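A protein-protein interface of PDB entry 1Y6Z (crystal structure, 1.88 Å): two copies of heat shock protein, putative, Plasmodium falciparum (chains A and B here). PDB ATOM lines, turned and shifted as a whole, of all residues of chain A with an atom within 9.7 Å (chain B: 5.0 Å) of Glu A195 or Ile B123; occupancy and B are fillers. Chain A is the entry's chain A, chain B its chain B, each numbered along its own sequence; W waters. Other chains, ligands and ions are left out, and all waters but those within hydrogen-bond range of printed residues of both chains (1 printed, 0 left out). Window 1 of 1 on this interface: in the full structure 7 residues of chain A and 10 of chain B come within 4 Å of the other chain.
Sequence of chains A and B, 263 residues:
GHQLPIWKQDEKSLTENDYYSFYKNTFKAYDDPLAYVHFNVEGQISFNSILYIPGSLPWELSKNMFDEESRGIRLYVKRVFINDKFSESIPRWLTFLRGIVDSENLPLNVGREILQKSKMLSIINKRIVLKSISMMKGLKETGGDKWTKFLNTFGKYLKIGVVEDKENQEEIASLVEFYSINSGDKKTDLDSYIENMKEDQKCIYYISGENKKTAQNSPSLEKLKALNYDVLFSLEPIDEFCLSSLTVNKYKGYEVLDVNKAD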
ATOM      1  N   LYS A 140      31.090 -33.014 -24.940  1.00  0.00           N
ATOM      2  CA  LYS A 140      30.136 -32.480 -23.982  1.00  0.00           C
ATOM      3  C   LYS A 140      28.722 -32.384 -24.571  1.00  0.00           C
ATOM      4  O   LYS A 140      27.717 -32.710 -23.915  1.00  0.00           O
ATOM      5  CB  LYS A 140      30.557 -31.054 -23.620  1.00  0.00           C
ATOM      6  CG  LYS A 140      29.749 -30.491 -22.457  1.00  0.00           C
ATOM      7  CD  LYS A 140      30.196 -29.097 -21.987  1.00  0.00           C
ATOM      8  CE  LYS A 140      29.060 -28.575 -21.108  1.00  0.00           C
ATOM      9  NZ  LYS A 140      29.479 -27.576 -20.082  1.00  0.00           N
ATOM     10  N   THR A 188      27.590 -29.472 -11.233  1.00  0.00           N
ATOM     11  CA  THR A 188      27.056 -28.521 -12.198  1.00  0.00           C
ATOM     12  C   THR A 188      28.197 -27.854 -12.993  1.00  0.00           C
ATOM     13  O   THR A 188      29.304 -27.625 -12.437  1.00  0.00           O
ATOM     14  CB  THR A 188      26.182 -27.418 -11.484  1.00  0.00           C
ATOM     15  OG1 THR A 188      25.757 -26.442 -12.453  1.00  0.00           O
ATOM     16  CG2 THR A 188      26.975 -26.697 -10.359  1.00  0.00           C
ATOM     17  N   ASP A 189      27.953 -27.511 -14.264  1.00  0.00           N
ATOM     18  CA  ASP A 189      28.845 -26.571 -14.962  1.00  0.00           C
ATOM     19  C   ASP A 189      28.480 -25.098 -14.592  1.00  0.00           C
ATOM     20  O   ASP A 189      27.461 -24.829 -13.944  1.00  0.00           O
ATOM     21  CB  ASP A 189      28.956 -26.852 -16.494  1.00  0.00           C
ATOM     22  CG  ASP A 189      27.640 -26.601 -17.267  1.00  0.00           C
ATOM     23  OD1 ASP A 189      26.740 -25.908 -16.736  1.00  0.00           O
ATOM     24  OD2 ASP A 189      27.551 -27.024 -18.458  1.00  0.00           O
ATOM     25  N   LEU A 190      29.338 -24.153 -14.964  1.00  0.00           N
ATOM     26  CA  LEU A 190      29.161 -22.772 -14.614  1.00  0.00           C
ATOM     27  C   LEU A 190      27.994 -22.132 -15.367  1.00  0.00           C
ATOM     28  O   LEU A 190      27.311 -21.277 -14.843  1.00  0.00           O
ATOM     29  CB  LEU A 190      30.445 -21.992 -14.925  1.00  0.00           C
ATOM     30  CG  LEU A 190      31.654 -22.351 -14.020  1.00  0.00           C
ATOM     31  CD1 LEU A 190      32.839 -21.483 -14.345  1.00  0.00           C
ATOM     32  CD2 LEU A 190      31.175 -22.212 -12.529  1.00  0.00           C
ATOM     33  N   ASP A 191      27.813 -22.490 -16.609  1.00  0.00           N
ATOM     34  CA  ASP A 191      26.701 -21.921 -17.362  1.00  0.00           C
ATOM     35  C   ASP A 191      25.359 -22.355 -16.759  1.00  0.00           C
ATOM     36  O   ASP A 191      24.403 -21.599 -16.765  1.00  0.00           O
ATOM     37  CB  ASP A 191      26.813 -22.368 -18.825  1.00  0.00           C
ATOM     38  CG  ASP A 191      27.936 -21.633 -19.583  1.00  0.00           C
ATOM     39  OD1 ASP A 191      28.365 -22.137 -20.652  1.00  0.00           O
ATOM     40  OD2 ASP A 191      28.417 -20.579 -19.112  1.00  0.00           O
ATOM     41  N   SER A 192      25.249 -23.584 -16.316  1.00  0.00           N
ATOM     42  CA  SER A 192      23.975 -23.973 -15.664  1.00  0.00           C
ATOM     43  C   SER A 192      23.757 -23.227 -14.372  1.00  0.00           C
ATOM     44  O   SER A 192      22.620 -22.843 -14.039  1.00  0.00           O
ATOM     45  CB  SER A 192      23.828 -25.456 -15.464  1.00  0.00           C
ATOM     46  OG  SER A 192      24.018 -26.160 -16.692  1.00  0.00           O
ATOM     47  N   TYR A 193      24.839 -23.021 -13.618  1.00  0.00           N
ATOM     48  CA  TYR A 193      24.763 -22.216 -12.412  1.00  0.00           C
ATOM     49  C   TYR A 193      24.206 -20.821 -12.769  1.00  0.00           C
ATOM     50  O   TYR A 193      23.258 -20.305 -12.108  1.00  0.00           O
ATOM     51  CB  TYR A 193      26.173 -22.131 -11.772  1.00  0.00           C
ATOM     52  CG  TYR A 193      26.189 -21.304 -10.503  1.00  0.00           C
ATOM     53  CD1 TYR A 193      26.198 -21.917  -9.229  1.00  0.00           C
ATOM     54  CD2 TYR A 193      26.149 -19.925 -10.573  1.00  0.00           C
ATOM     55  CE1 TYR A 193      26.223 -21.121  -8.055  1.00  0.00           C
ATOM     56  CE2 TYR A 193      26.102 -19.147  -9.443  1.00  0.00           C
ATOM     57  CZ  TYR A 193      26.180 -19.728  -8.199  1.00  0.00           C
ATOM     58  OH  TYR A 193      26.163 -18.865  -7.153  1.00  0.00           O
ATOM     59  N   ILE A 194      24.745 -20.197 -13.825  1.00  0.00           N
ATOM     60  CA  ILE A 194      24.291 -18.844 -14.249  1.00  0.00           C
ATOM     61  C   ILE A 194      22.779 -18.858 -14.548  1.00  0.00           C
ATOM     62  O   ILE A 194      22.028 -17.958 -14.091  1.00  0.00           O
ATOM     63  CB  ILE A 194      25.123 -18.298 -15.456  1.00  0.00           C
ATOM     64  CG1 ILE A 194      26.529 -17.925 -14.965  1.00  0.00           C
ATOM     65  CG2 ILE A 194      24.533 -17.003 -16.039  1.00  0.00           C
ATOM     66  CD1 ILE A 194      27.580 -17.738 -16.071  1.00  0.00           C
ATOM     67  N   GLU A 195      22.339 -19.855 -15.306  1.00  0.00           N
ATOM     68  CA  GLU A 195      20.925 -19.918 -15.746  1.00  0.00           C
ATOM     69  C   GLU A 195      20.063 -20.098 -14.502  1.00  0.00           C
ATOM     70  O   GLU A 195      18.931 -19.664 -14.479  1.00  0.00           O
ATOM     71  CB  GLU A 195      20.643 -21.146 -16.629  1.00  0.00           C
ATOM     72  CG  GLU A 195      21.297 -21.148 -17.969  1.00  0.00           C
ATOM     73  CD  GLU A 195      21.037 -22.420 -18.769  1.00  0.00           C
ATOM     74  OE1 GLU A 195      20.896 -22.300 -20.000  1.00  0.00           O
ATOM     75  OE2 GLU A 195      20.983 -23.521 -18.197  1.00  0.00           O
ATOM     76  N   ASN A 196      20.610 -20.741 -13.466  1.00  0.00           N
ATOM     77  CA  ASN A 196      19.855 -20.996 -12.237  1.00  0.00           C
ATOM     78  C   ASN A 196      19.868 -19.847 -11.229  1.00  0.00           C
ATOM     79  O   ASN A 196      19.189 -19.943 -10.184  1.00  0.00           O
ATOM     80  CB  ASN A 196      20.217 -22.355 -11.601  1.00  0.00           C
ATOM     81  CG  ASN A 196      19.840 -23.531 -12.474  1.00  0.00           C
ATOM     82  OD1 ASN A 196      18.818 -23.503 -13.151  1.00  0.00           O
ATOM     83  ND2 ASN A 196      20.647 -24.598 -12.443  1.00  0.00           N
ATOM     84  N   MET A 197      20.585 -18.763 -11.551  1.00  0.00           N
ATOM     85  CA  MET A 197      20.811 -17.614 -10.643  1.00  0.00           C
ATOM     86  C   MET A 197      19.494 -16.891 -10.421  1.00  0.00           C
ATOM     87  O   MET A 197      18.746 -16.635 -11.370  1.00  0.00           O
ATOM     88  CB  MET A 197      21.851 -16.609 -11.172  1.00  0.00           C
ATOM     89  CG  MET A 197      23.346 -16.988 -10.976  1.00  0.00           C
ATOM     90  SD  MET A 197      24.453 -15.822 -11.761  1.00  0.00           S
ATOM     91  CE  MET A 197      24.360 -14.481 -10.578  1.00  0.00           C
ATOM     92  N   LYS A 198      19.214 -16.614  -9.156  1.00  0.00           N
ATOM     93  CA  LYS A 198      17.939 -16.046  -8.725  1.00  0.00           C
ATOM     94  C   LYS A 198      17.814 -14.604  -9.209  1.00  0.00           C
ATOM     95  O   LYS A 198      18.802 -13.975  -9.586  1.00  0.00           O
ATOM     96  CB  LYS A 198      17.817 -16.181  -7.197  1.00  0.00           C
ATOM     97  CG  LYS A 198      16.606 -16.985  -6.756  1.00  0.00           C
ATOM     98  CD  LYS A 198      16.485 -18.337  -7.487  1.00  0.00           C
ATOM     99  CE  LYS A 198      16.922 -19.514  -6.617  1.00  0.00           C
ATOM    100  NZ  LYS A 198      15.785 -20.297  -6.030  1.00  0.00           N
ATOM    101  N   GLU A 199      16.588 -14.079  -9.224  1.00  0.00           N
ATOM    102  CA  GLU A 199      16.339 -12.780  -9.849  1.00  0.00           C
ATOM    103  C   GLU A 199      17.291 -11.665  -9.361  1.00  0.00           C
ATOM    104  O   GLU A 199      17.871 -10.949 -10.164  1.00  0.00           O
ATOM    105  CB  GLU A 199      14.849 -12.398  -9.716  1.00  0.00           C
ATOM    106  CG  GLU A 199      14.292 -11.538 -10.868  1.00  0.00           C
ATOM    107  CD  GLU A 199      13.629 -12.369 -11.990  1.00  0.00           C
ATOM    108  OE1 GLU A 199      12.376 -12.496 -11.976  1.00  0.00           O
ATOM    109  OE2 GLU A 199      14.355 -12.888 -12.883  1.00  0.00           O
ATOM    110  N   GLN A 201      20.294 -12.041  -7.799  1.00  0.00           N
ATOM    111  CA  GLN A 201      21.674 -12.488  -7.613  1.00  0.00           C
ATOM    112  C   GLN A 201      22.664 -11.876  -8.606  1.00  0.00           C
ATOM    113  O   GLN A 201      22.437 -11.922  -9.804  1.00  0.00           O
ATOM    114  CB  GLN A 201      21.730 -14.011  -7.679  1.00  0.00           C
ATOM    115  CG  GLN A 201      23.075 -14.578  -7.338  1.00  0.00           C
ATOM    116  CD  GLN A 201      23.117 -16.087  -7.366  1.00  0.00           C
ATOM    117  OE1 GLN A 201      22.076 -16.730  -7.360  1.00  0.00           O
ATOM    118  NE2 GLN A 201      24.303 -16.649  -7.416  1.00  0.00           N
ATOM    119  N   ILE A 204      28.629 -15.220  -8.782  1.00  0.00           N
ATOM    120  CA  ILE A 204      28.740 -16.673  -8.525  1.00  0.00           C
ATOM    121  C   ILE A 204      29.466 -16.880  -7.179  1.00  0.00           C
ATOM    122  O   ILE A 204      30.459 -16.261  -6.959  1.00  0.00           O
ATOM    123  CB  ILE A 204      29.520 -17.343  -9.674  1.00  0.00           C
ATOM    124  CG1 ILE A 204      28.781 -17.128 -11.005  1.00  0.00           C
ATOM    125  CG2 ILE A 204      29.697 -18.830  -9.406  1.00  0.00           C
ATOM    126  CD1 ILE A 204      29.707 -17.230 -12.293  1.00  0.00           C
ATOM    127  N   ASP A 230      22.540 -20.610  -4.826  1.00  0.00           N
ATOM    128  CA  ASP A 230      23.472 -21.716  -4.896  1.00  0.00           C
ATOM    129  C   ASP A 230      24.910 -21.223  -4.606  1.00  0.00           C
ATOM    130  O   ASP A 230      25.242 -20.024  -4.733  1.00  0.00           O
ATOM    131  CB  ASP A 230      23.406 -22.439  -6.255  1.00  0.00           C
ATOM    132  CG  ASP A 230      23.828 -23.933  -6.167  1.00  0.00           C
ATOM    133  OD1 ASP A 230      23.908 -24.605  -7.223  1.00  0.00           O
ATOM    134  OD2 ASP A 230      24.149 -24.439  -5.070  1.00  0.00           O
ATOM    135  N   TYR A 251      34.042 -14.691 -14.799  1.00  0.00           N
ATOM    136  CA  TYR A 251      33.622 -15.687 -15.729  1.00  0.00           C
ATOM    137  C   TYR A 251      32.411 -15.150 -16.428  1.00  0.00           C
ATOM    138  O   TYR A 251      31.356 -14.922 -15.798  1.00  0.00           O
ATOM    139  CB  TYR A 251      33.268 -17.016 -15.038  1.00  0.00           C
ATOM    140  CG  TYR A 251      32.671 -18.001 -16.028  1.00  0.00           C
ATOM    141  CD1 TYR A 251      33.490 -18.653 -16.970  1.00  0.00           C
ATOM    142  CD2 TYR A 251      31.299 -18.271 -16.048  1.00  0.00           C
ATOM    143  CE1 TYR A 251      32.950 -19.550 -17.908  1.00  0.00           C
ATOM    144  CE2 TYR A 251      30.752 -19.172 -17.012  1.00  0.00           C
ATOM    145  CZ  TYR A 251      31.578 -19.795 -17.914  1.00  0.00           C
ATOM    146  OH  TYR A 251      31.102 -20.683 -18.865  1.00  0.00           O
ATOM    147  N   LYS A 252      32.569 -14.994 -17.737  1.00  0.00           N
ATOM    148  CA  LYS A 252      31.551 -14.398 -18.604  1.00  0.00           C
ATOM    149  C   LYS A 252      30.949 -13.131 -17.993  1.00  0.00           C
ATOM    150  O   LYS A 252      29.751 -12.949 -18.077  1.00  0.00           O
ATOM    151  CB  LYS A 252      30.467 -15.411 -18.964  1.00  0.00           C
ATOM    152  CG  LYS A 252      31.010 -16.474 -19.912  1.00  0.00           C
ATOM    153  CD  LYS A 252      29.979 -17.555 -20.253  1.00  0.00           C
ATOM    154  CE  LYS A 252      30.602 -18.523 -21.296  1.00  0.00           C
ATOM    155  NZ  LYS A 252      29.591 -19.610 -21.673  1.00  0.00           N
ATOM    156  N   TYR A 254      30.836 -12.363 -14.808  1.00  0.00           N
ATOM    157  CA  TYR A 254      30.274 -12.550 -13.474  1.00  0.00           C
ATOM    158  C   TYR A 254      31.434 -12.622 -12.537  1.00  0.00           C
ATOM    159  O   TYR A 254      32.437 -13.268 -12.839  1.00  0.00           O
ATOM    160  CB  TYR A 254      29.434 -13.826 -13.345  1.00  0.00           C
ATOM    161  CG  TYR A 254      28.090 -13.763 -14.056  1.00  0.00           C
ATOM    162  CD1 TYR A 254      27.982 -14.201 -15.356  1.00  0.00           C
ATOM    163  CD2 TYR A 254      26.941 -13.273 -13.417  1.00  0.00           C
ATOM    164  CE1 TYR A 254      26.791 -14.147 -16.056  1.00  0.00           C
ATOM    165  CE2 TYR A 254      25.712 -13.230 -14.111  1.00  0.00           C
ATOM    166  CZ  TYR A 254      25.669 -13.674 -15.438  1.00  0.00           C
ATOM    167  OH  TYR A 254      24.507 -13.711 -16.184  1.00  0.00           O
ATOM    168  N   GLN B  44      15.108 -26.642 -14.304  1.00  0.00           N
ATOM    169  CA  GLN B  44      14.192 -25.586 -13.929  1.00  0.00           C
ATOM    170  C   GLN B  44      13.203 -24.998 -14.934  1.00  0.00           C
ATOM    171  O   GLN B  44      12.061 -24.756 -14.516  1.00  0.00           O
ATOM    172  CB  GLN B  44      14.880 -24.440 -13.163  1.00  0.00           C
ATOM    173  CG  GLN B  44      16.126 -23.881 -13.813  1.00  0.00           C
ATOM    174  CD  GLN B  44      16.244 -22.356 -13.729  1.00  0.00           C
ATOM    175  OE1 GLN B  44      17.054 -21.753 -14.449  1.00  0.00           O
ATOM    176  NE2 GLN B  44      15.456 -21.733 -12.855  1.00  0.00           N
ATOM    177  N   ILE B  45      13.502 -24.711 -16.215  1.00  0.00           N
ATOM    178  CA  ILE B  45      14.525 -25.188 -17.201  1.00  0.00           C
ATOM    179  C   ILE B  45      13.946 -26.178 -18.238  1.00  0.00           C
ATOM    180  O   ILE B  45      14.449 -26.266 -19.365  1.00  0.00           O
ATOM    181  CB  ILE B  45      16.042 -25.357 -16.775  1.00  0.00           C
ATOM    182  CG1 ILE B  45      16.868 -24.264 -17.472  1.00  0.00           C
ATOM    183  CG2 ILE B  45      16.622 -26.698 -17.215  1.00  0.00           C
ATOM    184  CD1 ILE B  45      18.061 -23.782 -16.720  1.00  0.00           C
ATOM    185  N   LYS B 119      14.127 -13.355 -18.155  1.00  0.00           N
ATOM    186  CA  LYS B 119      15.431 -13.989 -17.966  1.00  0.00           C
ATOM    187  C   LYS B 119      15.183 -15.467 -17.776  1.00  0.00           C
ATOM    188  O   LYS B 119      15.409 -15.998 -16.668  1.00  0.00           O
ATOM    189  CB  LYS B 119      16.139 -13.443 -16.715  1.00  0.00           C
ATOM    190  CG  LYS B 119      15.908 -11.955 -16.425  1.00  0.00           C
ATOM    191  CD  LYS B 119      16.723 -11.046 -17.341  1.00  0.00           C
ATOM    192  CE  LYS B 119      17.224  -9.810 -16.575  1.00  0.00           C
ATOM    193  NZ  LYS B 119      18.447 -10.093 -15.766  1.00  0.00           N
ATOM    194  N   MET B 120      14.767 -16.111 -18.876  1.00  0.00           N
ATOM    195  CA  MET B 120      14.081 -17.395 -18.883  1.00  0.00           C
ATOM    196  C   MET B 120      13.631 -17.758 -20.311  1.00  0.00           C
ATOM    197  O   MET B 120      13.888 -18.863 -20.831  1.00  0.00           O
ATOM    198  CB  MET B 120      12.859 -17.310 -17.977  1.00  0.00           C
ATOM    199  CG  MET B 120      12.319 -18.643 -17.556  1.00  0.00           C
ATOM    200  SD  MET B 120      11.496 -19.474 -18.920  1.00  0.00           S
ATOM    201  CE  MET B 120      12.185 -21.138 -18.792  1.00  0.00           C
ATOM    202  N   LEU B 121      12.917 -16.835 -20.943  1.00  0.00           N
ATOM    203  CA  LEU B 121      12.589 -17.001 -22.334  1.00  0.00           C
ATOM    204  C   LEU B 121      13.919 -16.869 -23.022  1.00  0.00           C
ATOM    205  O   LEU B 121      14.205 -17.547 -24.021  1.00  0.00           O
ATOM    206  CB  LEU B 121      11.672 -15.890 -22.794  1.00  0.00           C
ATOM    207  CG  LEU B 121      10.946 -16.199 -24.096  1.00  0.00           C
ATOM    208  CD1 LEU B 121       9.721 -17.046 -23.741  1.00  0.00           C
ATOM    209  CD2 LEU B 121      10.555 -14.906 -24.777  1.00  0.00           C
ATOM    210  N   SER B 122      14.726 -16.001 -22.423  1.00  0.00           N
ATOM    211  CA  SER B 122      16.056 -15.690 -22.844  1.00  0.00           C
ATOM    212  C   SER B 122      16.954 -16.948 -22.821  1.00  0.00           C
ATOM    213  O   SER B 122      17.804 -17.126 -23.682  1.00  0.00           O
ATOM    214  CB  SER B 122      16.600 -14.646 -21.899  1.00  0.00           C
ATOM    215  OG  SER B 122      17.807 -14.111 -22.371  1.00  0.00           O
ATOM    216  N   ILE B 123      16.773 -17.777 -21.803  1.00  0.00           N
ATOM    217  CA  ILE B 123      17.488 -19.037 -21.675  1.00  0.00           C
ATOM    218  C   ILE B 123      17.103 -19.993 -22.811  1.00  0.00           C
ATOM    219  O   ILE B 123      17.961 -20.613 -23.448  1.00  0.00           O
ATOM    220  CB  ILE B 123      17.144 -19.670 -20.332  1.00  0.00           C
ATOM    221  CG1 ILE B 123      18.012 -19.008 -19.243  1.00  0.00           C
ATOM    222  CG2 ILE B 123      17.286 -21.195 -20.387  1.00  0.00           C
ATOM    223  CD1 ILE B 123      17.403 -19.058 -17.890  1.00  0.00           C
ATOM    224  N   ILE B 124      15.805 -20.115 -23.047  1.00  0.00           N
ATOM    225  CA  ILE B 124      15.339 -20.977 -24.134  1.00  0.00           C
ATOM    226  C   ILE B 124      15.905 -20.473 -25.481  1.00  0.00           C
ATOM    227  O   ILE B 124      16.437 -21.277 -26.264  1.00  0.00           O
ATOM    228  CB  ILE B 124      13.792 -21.155 -24.150  1.00  0.00           C
ATOM    229  CG1 ILE B 124      13.340 -21.857 -22.855  1.00  0.00           C
ATOM    230  CG2 ILE B 124      13.358 -21.997 -25.364  1.00  0.00           C
ATOM    231  CD1 ILE B 124      11.837 -21.885 -22.643  1.00  0.00           C
ATOM    232  N   ASN B 125      15.792 -19.165 -25.735  1.00  0.00           N
ATOM    233  CA  ASN B 125      16.327 -18.537 -26.931  1.00  0.00           C
ATOM    234  C   ASN B 125      17.803 -18.846 -27.155  1.00  0.00           C
ATOM    235  O   ASN B 125      18.217 -19.208 -28.260  1.00  0.00           O
ATOM    236  CB  ASN B 125      16.127 -17.021 -26.888  1.00  0.00           C
ATOM    237  CG  ASN B 125      14.656 -16.622 -26.992  1.00  0.00           C
ATOM    238  OD1 ASN B 125      14.291 -15.487 -26.686  1.00  0.00           O
ATOM    239  ND2 ASN B 125      13.798 -17.580 -27.383  1.00  0.00           N
ATOM    240  N   LYS B 126      18.603 -18.673 -26.102  1.00  0.00           N
ATOM    241  CA  LYS B 126      20.032 -18.945 -26.197  1.00  0.00           C
ATOM    242  C   LYS B 126      20.360 -20.385 -26.585  1.00  0.00           C
ATOM    243  O   LYS B 126      21.242 -20.594 -27.365  1.00  0.00           O
ATOM    244  CB  LYS B 126      20.728 -18.581 -24.863  1.00  0.00           C
ATOM    245  CG  LYS B 126      22.211 -18.268 -25.091  1.00  0.00           C
ATOM    246  CD  LYS B 126      23.017 -18.362 -23.792  1.00  0.00           C
ATOM    247  CE  LYS B 126      24.439 -18.799 -24.128  1.00  0.00           C
ATOM    248  NZ  LYS B 126      25.375 -18.463 -23.010  1.00  0.00           N
ATOM    249  N   ARG B 127      19.639 -21.355 -26.020  1.00  0.00           N
ATOM    250  CA  ARG B 127      19.845 -22.796 -26.242  1.00  0.00           C
ATOM    251  C   ARG B 127      19.454 -23.105 -27.696  1.00  0.00           C
ATOM    252  O   ARG B 127      20.084 -23.910 -28.376  1.00  0.00           O
ATOM    253  CB  ARG B 127      18.874 -23.565 -25.365  1.00  0.00           C
ATOM    254  CG  ARG B 127      19.339 -24.388 -24.114  1.00  0.00           C
ATOM    255  CD  ARG B 127      20.367 -23.787 -23.246  1.00  0.00           C
ATOM    256  NE  ARG B 127      20.321 -24.272 -21.835  1.00  0.00           N
ATOM    257  CZ  ARG B 127      20.519 -25.528 -21.412  1.00  0.00           C
ATOM    258  NH1 ARG B 127      20.497 -25.802 -20.096  1.00  0.00           N
ATOM    259  NH2 ARG B 127      20.745 -26.526 -22.267  1.00  0.00           N
HETATM  260  O   HOH W   1      26.584 -21.094 -22.802  1.00  0.00           O
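O of Glu A195 sits close to OE1 of Gln B44 (2.8 Å). OE1 of Glu A195 is in salt-bridge range of NE of Arg B127, at 2.8 Å. The side-chain amide oxygen (OD1) of Asn A196 lies close to the side-chain amide oxygen (OE1) of Gln B44 (2.8 Å).
The backbone carbonyl oxygen (O) of Ser A192 lies within hydrogen-bond range of the side-chain amide nitrogen (ND2) of Asn A196 (3.1 Å).
Glu A195 touches Ile B45. Ile B123 touches Glu A195. Asn A196 touches Ile B45 (OD1 to CD1, 3.7 Å). Glu A199 touches Lys B119.
Of chain B, only Gln B44 (2.8 Å), Ile B45 (3.3 Å), Ile B123 (3.8 Å) and Arg B127 (2.8 Å) come within 4 Å of Glu A195. Ile B123 touches just one residue of chain A: Glu A195 (3.8 Å). No residue of chain A comes within 4 Å of Ser B122. No residue of chain A comes within 4 Å of Ile B124. Printed residues of chain B within 4 Å of Asn A196: Gln B44 (2.8 Å) and Ile B45 (3.7 Å). Of the printed residues of chain A, Lys B119 touches Glu A199. Of the printed residues of chain A, Arg B127 touches Glu A195 (2.8 Å). Asp A191 touches none of the printed residues of chain B. Thr A188 touches none of the printed residues of chain B. The nearest residue of chain A that does not touch Ile B123 is Asn A196 (5.7 Å).
Hydrophobic or aromatic side chains of chain B that line the printed part of chain A: Ile B45 and Ile B123. Along chain B the printed residues that touch a printed residue of chain A span positions 44 to 127. Among the printed residues, Asp or Glu carboxylates within 4 Å of a Lys or Arg side-chain nitrogen of the other chain: Glu A195 with Arg B127.
No position is printed for both chains.
Water W1 bridges the side-chain amino group of Lys B126 (2.9 Å) and the side-chain carboxylate of Asp A191 (3.0 Å).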
